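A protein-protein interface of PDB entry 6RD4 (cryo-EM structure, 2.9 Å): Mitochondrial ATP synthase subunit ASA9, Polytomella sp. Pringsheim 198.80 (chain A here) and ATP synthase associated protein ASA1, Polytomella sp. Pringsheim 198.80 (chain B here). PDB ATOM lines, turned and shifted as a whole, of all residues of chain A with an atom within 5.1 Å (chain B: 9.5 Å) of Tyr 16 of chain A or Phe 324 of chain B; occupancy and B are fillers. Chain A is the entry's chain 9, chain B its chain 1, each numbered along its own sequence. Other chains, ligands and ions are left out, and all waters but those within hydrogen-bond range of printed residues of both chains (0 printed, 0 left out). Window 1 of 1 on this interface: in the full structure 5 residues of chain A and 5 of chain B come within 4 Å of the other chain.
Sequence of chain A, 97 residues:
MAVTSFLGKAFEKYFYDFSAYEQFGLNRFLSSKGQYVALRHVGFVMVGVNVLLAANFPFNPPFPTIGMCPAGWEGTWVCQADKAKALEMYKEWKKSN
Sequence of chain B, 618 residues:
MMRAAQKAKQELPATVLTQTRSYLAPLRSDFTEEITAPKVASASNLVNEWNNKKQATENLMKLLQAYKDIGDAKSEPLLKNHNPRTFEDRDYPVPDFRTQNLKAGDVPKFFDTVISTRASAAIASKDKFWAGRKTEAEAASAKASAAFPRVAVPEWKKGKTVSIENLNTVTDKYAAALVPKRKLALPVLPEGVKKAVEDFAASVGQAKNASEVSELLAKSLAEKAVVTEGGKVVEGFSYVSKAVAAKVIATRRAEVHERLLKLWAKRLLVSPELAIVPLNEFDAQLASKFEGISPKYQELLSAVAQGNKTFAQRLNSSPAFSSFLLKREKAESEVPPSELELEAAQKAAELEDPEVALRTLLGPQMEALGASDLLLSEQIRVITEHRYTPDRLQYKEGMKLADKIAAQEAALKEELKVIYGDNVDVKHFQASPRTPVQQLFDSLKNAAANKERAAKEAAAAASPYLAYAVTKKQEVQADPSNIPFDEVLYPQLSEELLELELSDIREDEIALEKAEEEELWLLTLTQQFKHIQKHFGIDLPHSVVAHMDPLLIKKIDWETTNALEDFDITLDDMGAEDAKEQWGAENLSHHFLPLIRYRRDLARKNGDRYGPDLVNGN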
ATOM      1  N   GLY A   8      14.138 -18.824 -28.172  1.00  0.00           N
ATOM      2  CA  GLY A   8      12.800 -19.372 -28.254  1.00  0.00           C
ATOM      3  C   GLY A   8      12.334 -19.902 -26.915  1.00  0.00           C
ATOM      4  O   GLY A   8      11.174 -19.726 -26.540  1.00  0.00           O
ATOM      5  N   PHE A  11      11.988 -16.613 -24.798  1.00  0.00           N
ATOM      6  CA  PHE A  11      10.743 -15.919 -25.092  1.00  0.00           C
ATOM      7  C   PHE A  11       9.543 -16.707 -24.606  1.00  0.00           C
ATOM      8  O   PHE A  11       8.540 -16.112 -24.217  1.00  0.00           O
ATOM      9  CB  PHE A  11      10.609 -15.638 -26.585  1.00  0.00           C
ATOM     10  CG  PHE A  11       9.315 -14.996 -26.951  1.00  0.00           C
ATOM     11  CD1 PHE A  11       9.024 -13.722 -26.523  1.00  0.00           C
ATOM     12  CD2 PHE A  11       8.371 -15.677 -27.687  1.00  0.00           C
ATOM     13  CE1 PHE A  11       7.831 -13.136 -26.836  1.00  0.00           C
ATOM     14  CE2 PHE A  11       7.184 -15.086 -28.002  1.00  0.00           C
ATOM     15  CZ  PHE A  11       6.912 -13.820 -27.568  1.00  0.00           C
ATOM     16  N   GLU A  12       9.643 -18.038 -24.585  1.00  0.00           N
ATOM     17  CA  GLU A  12       8.555 -18.865 -24.082  1.00  0.00           C
ATOM     18  C   GLU A  12       8.302 -18.619 -22.605  1.00  0.00           C
ATOM     19  O   GLU A  12       7.153 -18.476 -22.179  1.00  0.00           O
ATOM     20  CB  GLU A  12       8.864 -20.334 -24.320  1.00  0.00           C
ATOM     21  CG  GLU A  12       7.795 -21.258 -23.817  1.00  0.00           C
ATOM     22  CD  GLU A  12       8.294 -22.657 -23.646  1.00  0.00           C
ATOM     23  OE1 GLU A  12       8.043 -23.241 -22.577  1.00  0.00           O
ATOM     24  OE2 GLU A  12       8.946 -23.171 -24.575  1.00  0.00           O
ATOM     25  N   LYS A  13       9.359 -18.550 -21.807  1.00  0.00           N
ATOM     26  CA  LYS A  13       9.178 -18.256 -20.397  1.00  0.00           C
ATOM     27  C   LYS A  13       9.165 -16.766 -20.108  1.00  0.00           C
ATOM     28  O   LYS A  13       8.957 -16.381 -18.958  1.00  0.00           O
ATOM     29  CB  LYS A  13      10.242 -18.966 -19.552  1.00  0.00           C
ATOM     30  CG  LYS A  13      11.692 -18.590 -19.797  1.00  0.00           C
ATOM     31  CD  LYS A  13      12.586 -19.419 -18.854  1.00  0.00           C
ATOM     32  CE  LYS A  13      14.080 -19.062 -18.909  1.00  0.00           C
ATOM     33  NZ  LYS A  13      14.802 -19.519 -20.125  1.00  0.00           N
ATOM     34  N   TYR A  14       9.348 -15.917 -21.113  1.00  0.00           N
ATOM     35  CA  TYR A  14       8.925 -14.537 -20.943  1.00  0.00           C
ATOM     36  C   TYR A  14       7.454 -14.365 -21.311  1.00  0.00           C
ATOM     37  O   TYR A  14       6.745 -13.564 -20.693  1.00  0.00           O
ATOM     38  CB  TYR A  14       9.802 -13.596 -21.773  1.00  0.00           C
ATOM     39  CG  TYR A  14       9.178 -12.242 -21.973  1.00  0.00           C
ATOM     40  CD1 TYR A  14       9.011 -11.366 -20.912  1.00  0.00           C
ATOM     41  CD2 TYR A  14       8.721 -11.853 -23.217  1.00  0.00           C
ATOM     42  CE1 TYR A  14       8.412 -10.147 -21.088  1.00  0.00           C
ATOM     43  CE2 TYR A  14       8.125 -10.637 -23.401  1.00  0.00           C
ATOM     44  CZ  TYR A  14       7.975  -9.791 -22.338  1.00  0.00           C
ATOM     45  OH  TYR A  14       7.383  -8.576 -22.540  1.00  0.00           O
ATOM     46  N   PHE A  15       6.975 -15.129 -22.291  1.00  0.00           N
ATOM     47  CA  PHE A  15       5.585 -15.017 -22.709  1.00  0.00           C
ATOM     48  C   PHE A  15       4.644 -15.571 -21.655  1.00  0.00           C
ATOM     49  O   PHE A  15       3.624 -14.955 -21.343  1.00  0.00           O
ATOM     50  CB  PHE A  15       5.380 -15.749 -24.033  1.00  0.00           C
ATOM     51  CG  PHE A  15       4.056 -15.511 -24.664  1.00  0.00           C
ATOM     52  CD1 PHE A  15       3.030 -16.415 -24.511  1.00  0.00           C
ATOM     53  CD2 PHE A  15       3.839 -14.399 -25.431  1.00  0.00           C
ATOM     54  CE1 PHE A  15       1.813 -16.198 -25.078  1.00  0.00           C
ATOM     55  CE2 PHE A  15       2.621 -14.186 -26.005  1.00  0.00           C
ATOM     56  CZ  PHE A  15       1.609 -15.087 -25.827  1.00  0.00           C
ATOM     57  N   TYR A  16       4.978 -16.714 -21.076  1.00  0.00           N
ATOM     58  CA  TYR A  16       3.959 -17.497 -20.395  1.00  0.00           C
ATOM     59  C   TYR A  16       3.864 -17.201 -18.907  1.00  0.00           C
ATOM     60  O   TYR A  16       2.820 -16.749 -18.429  1.00  0.00           O
ATOM     61  CB  TYR A  16       4.224 -18.979 -20.623  1.00  0.00           C
ATOM     62  CG  TYR A  16       3.534 -19.490 -21.842  1.00  0.00           C
ATOM     63  CD1 TYR A  16       4.250 -19.878 -22.953  1.00  0.00           C
ATOM     64  CD2 TYR A  16       2.161 -19.561 -21.887  1.00  0.00           C
ATOM     65  CE1 TYR A  16       3.621 -20.330 -24.061  1.00  0.00           C
ATOM     66  CE2 TYR A  16       1.528 -20.006 -22.989  1.00  0.00           C
ATOM     67  CZ  TYR A  16       2.260 -20.390 -24.072  1.00  0.00           C
ATOM     68  OH  TYR A  16       1.606 -20.842 -25.178  1.00  0.00           O
ATOM     69  N   ASP A  17       4.937 -17.446 -18.166  1.00  0.00           N
ATOM     70  CA  ASP A  17       4.874 -17.368 -16.718  1.00  0.00           C
ATOM     71  C   ASP A  17       5.492 -16.102 -16.151  1.00  0.00           C
ATOM     72  O   ASP A  17       5.177 -15.742 -15.014  1.00  0.00           O
ATOM     73  CB  ASP A  17       5.534 -18.606 -16.105  1.00  0.00           C
ATOM     74  CG  ASP A  17       6.832 -18.948 -16.771  1.00  0.00           C
ATOM     75  OD1 ASP A  17       7.243 -18.191 -17.663  1.00  0.00           O
ATOM     76  OD2 ASP A  17       7.420 -19.994 -16.439  1.00  0.00           O
ATOM     77  N   PHE A  18       6.349 -15.423 -16.909  1.00  0.00           N
ATOM     78  CA  PHE A  18       6.757 -14.062 -16.572  1.00  0.00           C
ATOM     79  C   PHE A  18       5.522 -13.190 -16.656  1.00  0.00           C
ATOM     80  O   PHE A  18       5.043 -12.887 -17.745  1.00  0.00           O
ATOM     81  CB  PHE A  18       7.824 -13.564 -17.536  1.00  0.00           C
ATOM     82  CG  PHE A  18       8.643 -12.411 -17.017  1.00  0.00           C
ATOM     83  CD1 PHE A  18       8.102 -11.135 -16.902  1.00  0.00           C
ATOM     84  CD2 PHE A  18       9.981 -12.595 -16.705  1.00  0.00           C
ATOM     85  CE1 PHE A  18       8.857 -10.089 -16.440  1.00  0.00           C
ATOM     86  CE2 PHE A  18      10.748 -11.550 -16.248  1.00  0.00           C
ATOM     87  CZ  PHE A  18      10.186 -10.295 -16.117  1.00  0.00           C
ATOM     88  N   PRO B 319       1.011 -32.796 -32.766  1.00  0.00           N
ATOM     89  CA  PRO B 319       1.841 -31.642 -33.114  1.00  0.00           C
ATOM     90  C   PRO B 319       1.190 -30.308 -32.844  1.00  0.00           C
ATOM     91  O   PRO B 319       1.882 -29.294 -32.851  1.00  0.00           O
ATOM     92  CB  PRO B 319       2.093 -31.843 -34.605  1.00  0.00           C
ATOM     93  CG  PRO B 319       1.976 -33.252 -34.804  1.00  0.00           C
ATOM     94  CD  PRO B 319       0.951 -33.750 -33.879  1.00  0.00           C
ATOM     95  N   ALA B 320      -0.114 -30.267 -32.616  1.00  0.00           N
ATOM     96  CA  ALA B 320      -0.784 -29.004 -32.377  1.00  0.00           C
ATOM     97  C   ALA B 320      -0.489 -28.452 -31.009  1.00  0.00           C
ATOM     98  O   ALA B 320      -0.526 -27.241 -30.820  1.00  0.00           O
ATOM     99  CB  ALA B 320      -2.279 -29.179 -32.517  1.00  0.00           C
ATOM    100  N   PHE B 321      -0.239 -29.310 -30.037  1.00  0.00           N
ATOM    101  CA  PHE B 321      -0.116 -28.880 -28.658  1.00  0.00           C
ATOM    102  C   PHE B 321       1.324 -28.686 -28.248  1.00  0.00           C
ATOM    103  O   PHE B 321       1.587 -28.257 -27.131  1.00  0.00           O
ATOM    104  CB  PHE B 321      -0.817 -29.872 -27.745  1.00  0.00           C
ATOM    105  CG  PHE B 321      -2.273 -29.631 -27.640  1.00  0.00           C
ATOM    106  CD1 PHE B 321      -2.805 -29.009 -26.547  1.00  0.00           C
ATOM    107  CD2 PHE B 321      -3.105 -29.982 -28.658  1.00  0.00           C
ATOM    108  CE1 PHE B 321      -4.138 -28.760 -26.478  1.00  0.00           C
ATOM    109  CE2 PHE B 321      -4.426 -29.745 -28.581  1.00  0.00           C
ATOM    110  CZ  PHE B 321      -4.942 -29.126 -27.491  1.00  0.00           C
ATOM    111  N   SER B 322       2.255 -28.994 -29.122  1.00  0.00           N
ATOM    112  CA  SER B 322       3.627 -28.569 -28.975  1.00  0.00           C
ATOM    113  C   SER B 322       3.882 -27.247 -29.664  1.00  0.00           C
ATOM    114  O   SER B 322       5.024 -26.792 -29.693  1.00  0.00           O
ATOM    115  CB  SER B 322       4.568 -29.615 -29.546  1.00  0.00           C
ATOM    116  OG  SER B 322       4.467 -29.630 -30.952  1.00  0.00           O
ATOM    117  N   SER B 323       2.859 -26.646 -30.259  1.00  0.00           N
ATOM    118  CA  SER B 323       2.990 -25.323 -30.828  1.00  0.00           C
ATOM    119  C   SER B 323       3.062 -24.300 -29.720  1.00  0.00           C
ATOM    120  O   SER B 323       2.734 -24.580 -28.571  1.00  0.00           O
ATOM    121  CB  SER B 323       1.827 -25.015 -31.748  1.00  0.00           C
ATOM    122  OG  SER B 323       1.883 -25.833 -32.888  1.00  0.00           O
ATOM    123  N   PHE B 324       3.470 -23.088 -30.086  1.00  0.00           N
ATOM    124  CA  PHE B 324       3.789 -22.079 -29.091  1.00  0.00           C
ATOM    125  C   PHE B 324       2.552 -21.615 -28.342  1.00  0.00           C
ATOM    126  O   PHE B 324       2.577 -21.484 -27.120  1.00  0.00           O
ATOM    127  CB  PHE B 324       4.478 -20.895 -29.750  1.00  0.00           C
ATOM    128  CG  PHE B 324       4.879 -19.838 -28.781  1.00  0.00           C
ATOM    129  CD1 PHE B 324       5.978 -20.017 -27.980  1.00  0.00           C
ATOM    130  CD2 PHE B 324       4.140 -18.686 -28.644  1.00  0.00           C
ATOM    131  CE1 PHE B 324       6.330 -19.075 -27.083  1.00  0.00           C
ATOM    132  CE2 PHE B 324       4.491 -17.755 -27.738  1.00  0.00           C
ATOM    133  CZ  PHE B 324       5.585 -17.951 -26.959  1.00  0.00           C
ATOM    134  N   LEU B 325       1.470 -21.355 -29.045  1.00  0.00           N
ATOM    135  CA  LEU B 325       0.285 -20.825 -28.390  1.00  0.00           C
ATOM    136  C   LEU B 325      -0.518 -21.882 -27.662  1.00  0.00           C
ATOM    137  O   LEU B 325      -1.457 -21.535 -26.948  1.00  0.00           O
ATOM    138  CB  LEU B 325      -0.602 -20.142 -29.413  1.00  0.00           C
ATOM    139  CG  LEU B 325       0.056 -18.953 -30.077  1.00  0.00           C
ATOM    140  CD1 LEU B 325      -0.742 -18.566 -31.268  1.00  0.00           C
ATOM    141  CD2 LEU B 325       0.114 -17.823 -29.093  1.00  0.00           C
ATOM    142  N   LEU B 326      -0.192 -23.154 -27.839  1.00  0.00           N
ATOM    143  CA  LEU B 326      -0.904 -24.232 -27.175  1.00  0.00           C
ATOM    144  C   LEU B 326       0.016 -25.057 -26.304  1.00  0.00           C
ATOM    145  O   LEU B 326      -0.334 -26.175 -25.944  1.00  0.00           O
ATOM    146  CB  LEU B 326      -1.582 -25.139 -28.194  1.00  0.00           C
ATOM    147  CG  LEU B 326      -2.802 -24.625 -28.925  1.00  0.00           C
ATOM    148  CD1 LEU B 326      -3.266 -25.687 -29.826  1.00  0.00           C
ATOM    149  CD2 LEU B 326      -3.850 -24.311 -27.934  1.00  0.00           C
ATOM    150  N   LYS B 327       1.178 -24.517 -25.944  1.00  0.00           N
ATOM    151  CA  LYS B 327       2.210 -25.327 -25.312  1.00  0.00           C
ATOM    152  C   LYS B 327       1.871 -25.649 -23.866  1.00  0.00           C
ATOM    153  O   LYS B 327       2.111 -26.766 -23.404  1.00  0.00           O
ATOM    154  CB  LYS B 327       3.547 -24.615 -25.397  1.00  0.00           C
ATOM    155  CG  LYS B 327       4.696 -25.547 -25.402  1.00  0.00           C
ATOM    156  CD  LYS B 327       5.974 -24.833 -25.715  1.00  0.00           C
ATOM    157  CE  LYS B 327       6.029 -24.449 -27.150  1.00  0.00           C
ATOM    158  NZ  LYS B 327       7.316 -23.837 -27.514  1.00  0.00           N
ATOM    159  N   ARG B 328       1.293 -24.668 -23.167  1.00  0.00           N
ATOM    160  CA  ARG B 328       0.913 -24.842 -21.739  1.00  0.00           C
ATOM    161  C   ARG B 328      -0.574 -25.204 -21.639  1.00  0.00           C
ATOM    162  O   ARG B 328      -1.166 -24.961 -20.569  1.00  0.00           O
ATOM    163  CB  ARG B 328       1.223 -23.568 -20.945  1.00  0.00           C
ATOM    164  CG  ARG B 328       2.707 -23.250 -20.838  1.00  0.00           C
ATOM    165  CD  ARG B 328       2.975 -22.022 -19.985  1.00  0.00           C
ATOM    166  NE  ARG B 328       4.394 -21.705 -19.903  1.00  0.00           N
ATOM    167  CZ  ARG B 328       5.245 -22.277 -19.058  1.00  0.00           C
ATOM    168  NH1 ARG B 328       4.821 -23.204 -18.217  1.00  0.00           N
ATOM    169  NH2 ARG B 328       6.516 -21.920 -19.059  1.00  0.00           N
ATOM    170  N   GLU B 329      -1.150 -25.762 -22.710  1.00  0.00           N
ATOM    171  CA  GLU B 329      -2.551 -26.140 -22.691  1.00  0.00           C
ATOM    172  C   GLU B 329      -2.703 -27.647 -22.614  1.00  0.00           C
ATOM    173  O   GLU B 329      -1.801 -28.410 -22.958  1.00  0.00           O
ATOM    174  CB  GLU B 329      -3.271 -25.618 -23.927  1.00  0.00           C
ATOM    175  CG  GLU B 329      -3.618 -24.169 -23.857  1.00  0.00           C
ATOM    176  CD  GLU B 329      -4.333 -23.816 -22.586  1.00  0.00           C
ATOM    177  OE1 GLU B 329      -3.888 -22.872 -21.907  1.00  0.00           O
ATOM    178  OE2 GLU B 329      -5.338 -24.479 -22.255  1.00  0.00           O
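The side-chain carboxylate of Glu 12 of chain A lies within salt-bridge range of the side-chain amino group of Lys 327 of chain B (3.4 Å). The guanidinium group of Arg 328 of chain B is in salt-bridge range of the side-chain carboxylate of Asp 17 of chain A (3.4 Å). OH of Tyr 16 of chain A sits close to O of Phe 324 of chain B, at 2.3 Å.
Among the printed residues, pairs that only touch across the chains: Tyr 16 of chain A with Arg 328 of chain B, Tyr 16 of chain A with Leu 325 of chain B, Phe 11 of chain A with Phe 324 of chain B, Phe 15 of chain A with Phe 324 of chain B, Glu 12 of chain A with Phe 324 of chain B, Tyr 16 of chain A with Lys 327 of chain B and Tyr 16 of chain A with Leu 326 of chain B.
Of the printed residues of chain B, Phe 11 of chain A touches Phe 324 (3.4 Å). Printed residues of chain B within 4 Å of Glu 12 of chain A: Phe 324 (3.7 Å) and Lys 327 (3.4 Å). Lys 13 of chain A touches none of the printed residues of chain B. Of the printed residues of chain B, Phe 15 of chain A touches Phe 324 (3.7 Å). Of chain B, only Phe 324 (2.3 Å), Leu 325 (3.4 Å), Leu 326 (3.96 Å), Lys 327 (3.8 Å) and Arg 328 (2.8 Å) come within 4 Å of Tyr 16 of chain A. Pro 319 of chain B touches none of the printed residues of chain A. Of chain A, only Phe 11 (3.4 Å), Glu 12 (3.7 Å), Phe 15 (3.7 Å) and Tyr 16 (2.3 Å) come within 4 Å of Phe 324 of chain B. Printed residues of chain A within 4 Å of Leu 325 of chain B: Tyr 16. Printed residues of chain A within 4 Å of Arg 328 of chain B: Tyr 16 and Asp 17.
Of the 11 printed residues of chain B, 5 touch a printed residue of chain A. Hydrophobic or aromatic side chains of chain B within 4 Å of the printed part of chain A: Phe 324. Of the 9 printed residues of chain A, 5 touch a printed residue of chain B. Among the printed residues, 10 pairs touch across the chains.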
